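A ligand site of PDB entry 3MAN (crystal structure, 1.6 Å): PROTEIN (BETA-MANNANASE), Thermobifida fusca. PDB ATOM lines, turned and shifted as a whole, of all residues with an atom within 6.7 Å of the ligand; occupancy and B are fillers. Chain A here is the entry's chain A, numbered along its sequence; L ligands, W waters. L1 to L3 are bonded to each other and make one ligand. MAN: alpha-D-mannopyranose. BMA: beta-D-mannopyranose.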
ATOM      1  N   PRO A  27     -28.116 -14.789 -18.322  1.00  0.00           N
ATOM      2  CA  PRO A  27     -27.503 -13.565 -18.819  1.00  0.00           C
ATOM      3  C   PRO A  27     -28.380 -12.331 -18.691  1.00  0.00           C
ATOM      4  O   PRO A  27     -28.700 -11.658 -19.687  1.00  0.00           O
ATOM      5  CB  PRO A  27     -27.217 -13.919 -20.275  1.00  0.00           C
ATOM      6  CG  PRO A  27     -28.357 -14.828 -20.648  1.00  0.00           C
ATOM      7  CD  PRO A  27     -28.515 -15.705 -19.428  1.00  0.00           C
ATOM      8  N   ASN A  29     -27.919  -9.202 -17.659  1.00  0.00           N
ATOM      9  CA  ASN A  29     -27.494  -7.904 -18.177  1.00  0.00           C
ATOM     10  C   ASN A  29     -27.779  -7.741 -19.661  1.00  0.00           C
ATOM     11  O   ASN A  29     -28.161  -6.649 -20.130  1.00  0.00           O
ATOM     12  CB  ASN A  29     -25.990  -7.699 -17.953  1.00  0.00           C
ATOM     13  CG  ASN A  29     -25.555  -6.329 -18.430  1.00  0.00           C
ATOM     14  OD1 ASN A  29     -25.018  -6.228 -19.539  1.00  0.00           O
ATOM     15  ND2 ASN A  29     -25.822  -5.306 -17.619  1.00  0.00           N
ATOM     16  N   TRP A  30     -27.570  -8.808 -20.433  1.00  0.00           N
ATOM     17  CA  TRP A  30     -27.687  -8.730 -21.877  1.00  0.00           C
ATOM     18  C   TRP A  30     -29.094  -8.938 -22.383  1.00  0.00           C
ATOM     19  O   TRP A  30     -29.416  -8.605 -23.531  1.00  0.00           O
ATOM     20  CB  TRP A  30     -26.711  -9.735 -22.539  1.00  0.00           C
ATOM     21  CG  TRP A  30     -25.310  -9.512 -22.006  1.00  0.00           C
ATOM     22  CD1 TRP A  30     -24.683  -8.304 -21.832  1.00  0.00           C
ATOM     23  CD2 TRP A  30     -24.377 -10.515 -21.568  1.00  0.00           C
ATOM     24  NE1 TRP A  30     -23.427  -8.498 -21.328  1.00  0.00           N
ATOM     25  CE2 TRP A  30     -23.214  -9.841 -21.144  1.00  0.00           C
ATOM     26  CE3 TRP A  30     -24.428 -11.901 -21.510  1.00  0.00           C
ATOM     27  CZ2 TRP A  30     -22.097 -10.521 -20.666  1.00  0.00           C
ATOM     28  CZ3 TRP A  30     -23.314 -12.578 -21.013  1.00  0.00           C
ATOM     29  CH2 TRP A  30     -22.176 -11.879 -20.597  1.00  0.00           C
ATOM     30  N   TYR A  31     -29.953  -9.529 -21.573  1.00  0.00           N
ATOM     31  CA  TYR A  31     -31.332  -9.860 -21.932  1.00  0.00           C
ATOM     32  C   TYR A  31     -32.261  -9.500 -20.782  1.00  0.00           C
ATOM     33  O   TYR A  31     -32.924 -10.345 -20.199  1.00  0.00           O
ATOM     34  CB  TYR A  31     -31.426 -11.387 -22.196  1.00  0.00           C
ATOM     35  CG  TYR A  31     -30.623 -11.860 -23.379  1.00  0.00           C
ATOM     36  CD1 TYR A  31     -31.103 -11.812 -24.671  1.00  0.00           C
ATOM     37  CD2 TYR A  31     -29.333 -12.366 -23.189  1.00  0.00           C
ATOM     38  CE1 TYR A  31     -30.345 -12.240 -25.734  1.00  0.00           C
ATOM     39  CE2 TYR A  31     -28.568 -12.782 -24.253  1.00  0.00           C
ATOM     40  CZ  TYR A  31     -29.078 -12.738 -25.538  1.00  0.00           C
ATOM     41  OH  TYR A  31     -28.299 -13.188 -26.574  1.00  0.00           O
ATOM     42  N   PRO A  32     -32.401  -8.212 -20.455  1.00  0.00           N
ATOM     43  CA  PRO A  32     -33.237  -7.773 -19.364  1.00  0.00           C
ATOM     44  C   PRO A  32     -34.713  -8.072 -19.569  1.00  0.00           C
ATOM     45  O   PRO A  32     -35.495  -8.137 -18.626  1.00  0.00           O
ATOM     46  CB  PRO A  32     -33.010  -6.268 -19.301  1.00  0.00           C
ATOM     47  CG  PRO A  32     -32.511  -5.892 -20.665  1.00  0.00           C
ATOM     48  CD  PRO A  32     -31.671  -7.081 -21.072  1.00  0.00           C
ATOM     49  N   GLN A  33     -35.134  -8.282 -20.810  1.00  0.00           N
ATOM     50  CA  GLN A  33     -36.518  -8.592 -21.163  1.00  0.00           C
ATOM     51  C   GLN A  33     -36.921 -10.006 -20.787  1.00  0.00           C
ATOM     52  O   GLN A  33     -38.101 -10.357 -20.793  1.00  0.00           O
ATOM     53  CB  GLN A  33     -36.742  -8.411 -22.671  1.00  0.00           C
ATOM     54  CG  GLN A  33     -36.052  -9.343 -23.645  1.00  0.00           C
ATOM     55  CD  GLN A  33     -34.643  -8.978 -24.014  1.00  0.00           C
ATOM     56  OE1 GLN A  33     -34.030  -8.119 -23.368  1.00  0.00           O
ATOM     57  NE2 GLN A  33     -34.089  -9.567 -25.064  1.00  0.00           N
ATOM     58  N   ARG A  58     -17.594  -2.374 -19.181  1.00  0.00           N
ATOM     59  CA  ARG A  58     -17.691  -2.876 -20.540  1.00  0.00           C
ATOM     60  C   ARG A  58     -19.138  -2.861 -21.026  1.00  0.00           C
ATOM     61  O   ARG A  58     -19.376  -2.611 -22.209  1.00  0.00           O
ATOM     62  CB  ARG A  58     -17.161  -4.305 -20.692  1.00  0.00           C
ATOM     63  CG  ARG A  58     -15.708  -4.406 -21.104  1.00  0.00           C
ATOM     64  CD  ARG A  58     -15.361  -5.841 -21.437  1.00  0.00           C
ATOM     65  NE  ARG A  58     -15.833  -6.301 -22.740  1.00  0.00           N
ATOM     66  CZ  ARG A  58     -15.722  -7.586 -23.082  1.00  0.00           C
ATOM     67  NH1 ARG A  58     -15.200  -8.480 -22.254  1.00  0.00           N
ATOM     68  NH2 ARG A  58     -16.133  -8.022 -24.266  1.00  0.00           N
ATOM     69  N   TRP A  59     -20.096  -3.161 -20.165  1.00  0.00           N
ATOM     70  CA  TRP A  59     -21.508  -3.181 -20.547  1.00  0.00           C
ATOM     71  C   TRP A  59     -22.275  -2.090 -19.806  1.00  0.00           C
ATOM     72  O   TRP A  59     -21.640  -1.191 -19.244  1.00  0.00           O
ATOM     73  CB  TRP A  59     -22.120  -4.576 -20.351  1.00  0.00           C
ATOM     74  CG  TRP A  59     -21.462  -5.569 -21.289  1.00  0.00           C
ATOM     75  CD1 TRP A  59     -21.678  -5.666 -22.629  1.00  0.00           C
ATOM     76  CD2 TRP A  59     -20.474  -6.564 -20.977  1.00  0.00           C
ATOM     77  NE1 TRP A  59     -20.906  -6.647 -23.183  1.00  0.00           N
ATOM     78  CE2 TRP A  59     -20.137  -7.212 -22.174  1.00  0.00           C
ATOM     79  CE3 TRP A  59     -19.848  -6.947 -19.794  1.00  0.00           C
ATOM     80  CZ2 TRP A  59     -19.216  -8.258 -22.233  1.00  0.00           C
ATOM     81  CZ3 TRP A  59     -18.919  -7.981 -19.853  1.00  0.00           C
ATOM     82  CH2 TRP A  59     -18.615  -8.608 -21.069  1.00  0.00           C
ATOM     83  N   HIS A  86     -19.622  -9.188 -14.547  1.00  0.00           N
ATOM     84  CA  HIS A  86     -18.972  -9.845 -15.673  1.00  0.00           C
ATOM     85  C   HIS A  86     -17.847  -9.056 -16.308  1.00  0.00           C
ATOM     86  O   HIS A  86     -16.989  -9.576 -17.024  1.00  0.00           O
ATOM     87  CB  HIS A  86     -20.022 -10.195 -16.745  1.00  0.00           C
ATOM     88  CG  HIS A  86     -19.705 -11.460 -17.459  1.00  0.00           C
ATOM     89  ND1 HIS A  86     -20.091 -12.691 -16.955  1.00  0.00           N
ATOM     90  CD2 HIS A  86     -19.074 -11.707 -18.642  1.00  0.00           C
ATOM     91  CE1 HIS A  86     -19.665 -13.634 -17.774  1.00  0.00           C
ATOM     92  NE2 HIS A  86     -19.081 -13.066 -18.817  1.00  0.00           N
ATOM     93  N   THR A  89     -13.876  -9.944 -16.744  1.00  0.00           N
ATOM     94  CA  THR A  89     -13.462 -11.074 -17.555  1.00  0.00           C
ATOM     95  C   THR A  89     -12.211 -10.815 -18.383  1.00  0.00           C
ATOM     96  O   THR A  89     -12.179  -9.936 -19.245  1.00  0.00           O
ATOM     97  CB  THR A  89     -14.599 -11.529 -18.491  1.00  0.00           C
ATOM     98  OG1 THR A  89     -15.771 -11.828 -17.736  1.00  0.00           O
ATOM     99  CG2 THR A  89     -14.234 -12.755 -19.326  1.00  0.00           C
ATOM    100  N   ASN A 127     -16.233 -12.045 -12.426  1.00  0.00           N
ATOM    101  CA  ASN A 127     -16.074 -13.211 -13.282  1.00  0.00           C
ATOM    102  C   ASN A 127     -14.662 -13.312 -13.875  1.00  0.00           C
ATOM    103  O   ASN A 127     -14.092 -12.311 -14.303  1.00  0.00           O
ATOM    104  CB  ASN A 127     -17.003 -13.080 -14.504  1.00  0.00           C
ATOM    105  CG  ASN A 127     -17.014 -14.288 -15.411  1.00  0.00           C
ATOM    106  OD1 ASN A 127     -16.681 -14.286 -16.619  1.00  0.00           O
ATOM    107  ND2 ASN A 127     -17.387 -15.415 -14.860  1.00  0.00           N
ATOM    108  N   GLU A 128     -14.079 -14.495 -13.873  1.00  0.00           N
ATOM    109  CA  GLU A 128     -12.796 -14.819 -14.532  1.00  0.00           C
ATOM    110  C   GLU A 128     -11.900 -13.610 -14.624  1.00  0.00           C
ATOM    111  O   GLU A 128     -11.598 -13.111 -15.691  1.00  0.00           O
ATOM    112  CB  GLU A 128     -13.183 -15.283 -15.944  1.00  0.00           C
ATOM    113  CG  GLU A 128     -14.036 -16.542 -15.939  1.00  0.00           C
ATOM    114  CD  GLU A 128     -14.422 -17.097 -17.285  1.00  0.00           C
ATOM    115  OE1 GLU A 128     -14.075 -16.447 -18.307  1.00  0.00           O
ATOM    116  OE2 GLU A 128     -15.024 -18.197 -17.349  1.00  0.00           O
ATOM    117  N   TRP A 254     -23.170 -23.358 -17.593  1.00  0.00           N
ATOM    118  CA  TRP A 254     -23.298 -22.168 -18.458  1.00  0.00           C
ATOM    119  C   TRP A 254     -23.923 -22.636 -19.762  1.00  0.00           C
ATOM    120  O   TRP A 254     -23.374 -23.548 -20.382  1.00  0.00           O
ATOM    121  CB  TRP A 254     -21.902 -21.558 -18.724  1.00  0.00           C
ATOM    122  CG  TRP A 254     -21.973 -20.330 -19.606  1.00  0.00           C
ATOM    123  CD1 TRP A 254     -22.061 -20.292 -20.968  1.00  0.00           C
ATOM    124  CD2 TRP A 254     -22.010 -18.970 -19.162  1.00  0.00           C
ATOM    125  NE1 TRP A 254     -22.174 -18.987 -21.398  1.00  0.00           N
ATOM    126  CE2 TRP A 254     -22.126 -18.152 -20.313  1.00  0.00           C
ATOM    127  CE3 TRP A 254     -21.968 -18.343 -17.912  1.00  0.00           C
ATOM    128  CZ2 TRP A 254     -22.223 -16.764 -20.261  1.00  0.00           C
ATOM    129  CZ3 TRP A 254     -22.063 -16.964 -17.858  1.00  0.00           C
ATOM    130  CH2 TRP A 254     -22.191 -16.182 -19.017  1.00  0.00           C
ATOM    131  N   SER A 255     -25.018 -22.055 -20.241  1.00  0.00           N
ATOM    132  CA  SER A 255     -25.818 -21.065 -19.560  1.00  0.00           C
ATOM    133  C   SER A 255     -27.271 -21.259 -20.054  1.00  0.00           C
ATOM    134  O   SER A 255     -27.536 -22.027 -21.009  1.00  0.00           O
ATOM    135  CB  SER A 255     -25.412 -19.623 -19.847  1.00  0.00           C
ATOM    136  OG  SER A 255     -25.605 -19.371 -21.229  1.00  0.00           O
ATOM    137  N   GLY A 258     -29.219 -17.694 -24.991  1.00  0.00           N
ATOM    138  CA  GLY A 258     -28.696 -16.462 -25.524  1.00  0.00           C
ATOM    139  C   GLY A 258     -27.227 -16.309 -25.759  1.00  0.00           C
ATOM    140  O   GLY A 258     -26.726 -15.196 -25.908  1.00  0.00           O
ATOM    141  N   ASN A 259     -26.472 -17.406 -25.805  1.00  0.00           N
ATOM    142  CA  ASN A 259     -25.058 -17.304 -26.091  1.00  0.00           C
ATOM    143  C   ASN A 259     -24.819 -16.746 -27.494  1.00  0.00           C
ATOM    144  O   ASN A 259     -25.536 -17.099 -28.422  1.00  0.00           O
ATOM    145  CB  ASN A 259     -24.349 -18.659 -25.980  1.00  0.00           C
ATOM    146  CG  ASN A 259     -24.109 -18.981 -24.519  1.00  0.00           C
ATOM    147  OD1 ASN A 259     -23.204 -18.421 -23.892  1.00  0.00           O
ATOM    148  ND2 ASN A 259     -24.924 -19.863 -23.985  1.00  0.00           N
ATOM    149  N   GLY A 260     -23.752 -15.977 -27.623  1.00  0.00           N
ATOM    150  CA  GLY A 260     -23.273 -15.427 -28.875  1.00  0.00           C
ATOM    151  C   GLY A 260     -21.769 -15.716 -28.962  1.00  0.00           C
ATOM    152  O   GLY A 260     -21.319 -16.699 -28.316  1.00  0.00           O
ATOM    153  N   GLY A 261     -21.016 -15.047 -29.800  1.00  0.00           N
ATOM    154  CA  GLY A 261     -19.591 -15.276 -29.930  1.00  0.00           C
ATOM    155  C   GLY A 261     -19.111 -16.671 -30.238  1.00  0.00           C
ATOM    156  O   GLY A 261     -18.008 -17.021 -29.805  1.00  0.00           O
ATOM    157  N   GLY A 262     -19.842 -17.490 -30.992  1.00  0.00           N
ATOM    158  CA  GLY A 262     -19.419 -18.817 -31.371  1.00  0.00           C
ATOM    159  C   GLY A 262     -19.592 -19.879 -30.297  1.00  0.00           C
ATOM    160  O   GLY A 262     -18.993 -20.957 -30.361  1.00  0.00           O
ATOM    161  N   VAL A 263     -20.420 -19.612 -29.302  1.00  0.00           N
ATOM    162  CA  VAL A 263     -20.611 -20.567 -28.187  1.00  0.00           C
ATOM    163  C   VAL A 263     -22.074 -20.898 -28.025  1.00  0.00           C
ATOM    164  O   VAL A 263     -22.625 -21.232 -26.983  1.00  0.00           O
ATOM    165  CB  VAL A 263     -19.836 -19.950 -27.015  1.00  0.00           C
ATOM    166  CG1 VAL A 263     -20.513 -19.868 -25.670  1.00  0.00           C
ATOM    167  CG2 VAL A 263     -18.495 -20.706 -26.890  1.00  0.00           C
ATOM    168  N   LEU A 266     -23.729 -23.834 -26.048  1.00  0.00           N
ATOM    169  CA  LEU A 266     -23.873 -23.788 -24.613  1.00  0.00           C
ATOM    170  C   LEU A 266     -25.247 -23.311 -24.155  1.00  0.00           C
ATOM    171  O   LEU A 266     -25.518 -23.262 -22.956  1.00  0.00           O
ATOM    172  CB  LEU A 266     -22.746 -22.984 -23.959  1.00  0.00           C
ATOM    173  CG  LEU A 266     -21.331 -23.532 -24.121  1.00  0.00           C
ATOM    174  CD1 LEU A 266     -20.308 -22.585 -23.537  1.00  0.00           C
ATOM    175  CD2 LEU A 266     -21.242 -24.903 -23.470  1.00  0.00           C
HETATM  176  C1  MAN L   1     -19.421 -16.008 -24.091  1.00  0.00           C
HETATM  177  C2  MAN L   1     -20.850 -15.969 -24.690  1.00  0.00           C
HETATM  178  C3  MAN L   1     -21.014 -14.597 -25.322  1.00  0.00           C
HETATM  179  C4  MAN L   1     -20.707 -13.620 -24.240  1.00  0.00           C
HETATM  180  C5  MAN L   1     -19.302 -13.703 -23.628  1.00  0.00           C
HETATM  181  C6  MAN L   1     -19.127 -12.622 -22.573  1.00  0.00           C
HETATM  182  O2  MAN L   1     -21.876 -16.123 -23.699  1.00  0.00           O
HETATM  183  O3  MAN L   1     -22.360 -14.416 -25.746  1.00  0.00           O
HETATM  184  O4  MAN L   1     -20.864 -12.263 -24.736  1.00  0.00           O
HETATM  185  O5  MAN L   1     -19.265 -15.011 -23.077  1.00  0.00           O
HETATM  186  O6  MAN L   1     -17.912 -12.863 -21.893  1.00  0.00           O
HETATM  187  C1  BMA L   2     -21.878 -11.237 -24.637  1.00  0.00           C
HETATM  188  C2  BMA L   2     -21.504  -9.790 -25.084  1.00  0.00           C
HETATM  189  C3  BMA L   2     -22.826  -9.084 -24.942  1.00  0.00           C
HETATM  190  C4  BMA L   2     -23.738  -9.865 -25.802  1.00  0.00           C
HETATM  191  C5  BMA L   2     -24.049 -11.323 -25.425  1.00  0.00           C
HETATM  192  C6  BMA L   2     -25.013 -12.080 -26.327  1.00  0.00           C
HETATM  193  O2  BMA L   2     -21.062  -9.936 -26.416  1.00  0.00           O
HETATM  194  O3  BMA L   2     -22.638  -7.742 -25.371  1.00  0.00           O
HETATM  195  O4  BMA L   2     -25.043  -9.278 -25.761  1.00  0.00           O
HETATM  196  O5  BMA L   2     -22.776 -11.934 -25.508  1.00  0.00           O
HETATM  197  O6  BMA L   2     -24.714 -11.789 -27.668  1.00  0.00           O
HETATM  198  C1  BMA L   3     -25.860  -8.678 -27.029  1.00  0.00           C
HETATM  199  C2  BMA L   3     -27.262  -8.119 -26.651  1.00  0.00           C
HETATM  200  C3  BMA L   3     -27.531  -7.128 -27.772  1.00  0.00           C
HETATM  201  C4  BMA L   3     -26.514  -6.012 -27.769  1.00  0.00           C
HETATM  202  C5  BMA L   3     -25.118  -6.663 -28.021  1.00  0.00           C
HETATM  203  C6  BMA L   3     -23.982  -5.681 -28.080  1.00  0.00           C
HETATM  204  O2  BMA L   3     -27.169  -7.558 -25.363  1.00  0.00           O
HETATM  205  O3  BMA L   3     -28.848  -6.701 -27.524  1.00  0.00           O
HETATM  206  O4  BMA L   3     -26.771  -5.057 -28.759  1.00  0.00           O
HETATM  207  O5  BMA L   3     -24.882  -7.636 -26.990  1.00  0.00           O
HETATM  208  O6  BMA L   3     -23.489  -5.711 -26.758  1.00  0.00           O
HETATM  209  O   HOH W   1     -21.904 -11.936 -28.321  1.00  0.00           O
HETATM  210  O   HOH W   2     -17.640 -15.062 -20.540  1.00  0.00           O
HETATM  211  O   HOH W   3     -25.111  -5.295 -24.005  1.00  0.00           O
HETATM  212  O   HOH W   4     -24.522 -14.853 -23.403  1.00  0.00           O
HETATM  213  O   HOH W   5     -19.384  -6.933 -26.024  1.00  0.00           O
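An oxygen (O2) of MAN L1 lies within hydrogen-bond range of the side-chain amide oxygen of Asn 259 (2.7 Å). The indole nitrogen (NE1) of Trp 59 lies within hydrogen-bond range of an oxygen (O3) of BMA L2. The backbone carbonyl oxygen of Trp 30 sits at hydrogen-bond distance from an oxygen (O2) of BMA L3 (3.1 Å). O6 of MAN L1 lies within hydrogen-bond range of NE2 of His 86 (3.3 Å). An oxygen (O3) of MAN L1 sits at hydrogen-bond distance from the backbone NH of Gly 260 (2.8 Å).
The indole nitrogen (NE1) of Trp 30 sits close to the side-chain amide oxygen (OD1) of Asn 29. OG of Ser 255 is in hydrogen-bond range of NE1 of Trp 254 (3.5 Å). OG of Ser 255 lies within hydrogen-bond range of ND2 of Asn 259. OH of Tyr 31 is in hydrogen-bond range of O of Gly 258, at 2.6 Å. OD1 of Asn 259 is in hydrogen-bond range of NE1 of Trp 254 (2.8 Å). A ring nitrogen (NE2) of His 86 sits close to the side-chain amide oxygen of Asn 127. The backbone carbonyl oxygen (O) of His 86 sits at hydrogen-bond distance from the side-chain hydroxyl (OG1) of Thr 89 (2.7 Å).
Residues that only touch the ligand: Tyr 31 (3.5 Å), Trp 254 (3.5 Å) and Gly 258 (3.6 Å). Hydrophobic or aromatic side chains that line the ligand: Trp 30, Trp 59, His 86 and Trp 254. Within 4 Å of the ligand: Trp 30, Tyr 31, Trp 59, His 86, Trp 254, Gly 258, Asn 259 and Gly 260. Along chain A the residues within 4 Å of the ligand span positions 30 to 260. The nearest printed residue that does not touch the ligand is Val 263 (4.03 Å).
Water W2 lies within hydrogen-bond range of O6 of MAN L1 (2.6 Å) and NE2 of His 86 (3.0 Å). Water W4 lies within hydrogen-bond range of an oxygen (O2) of MAN L1 (2.9 Å) and the backbone carbonyl oxygen (O) of Gly 258 (3.4 Å). Water W5 bridges the indole nitrogen of Trp 59 and an oxygen (O3) of BMA L2.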
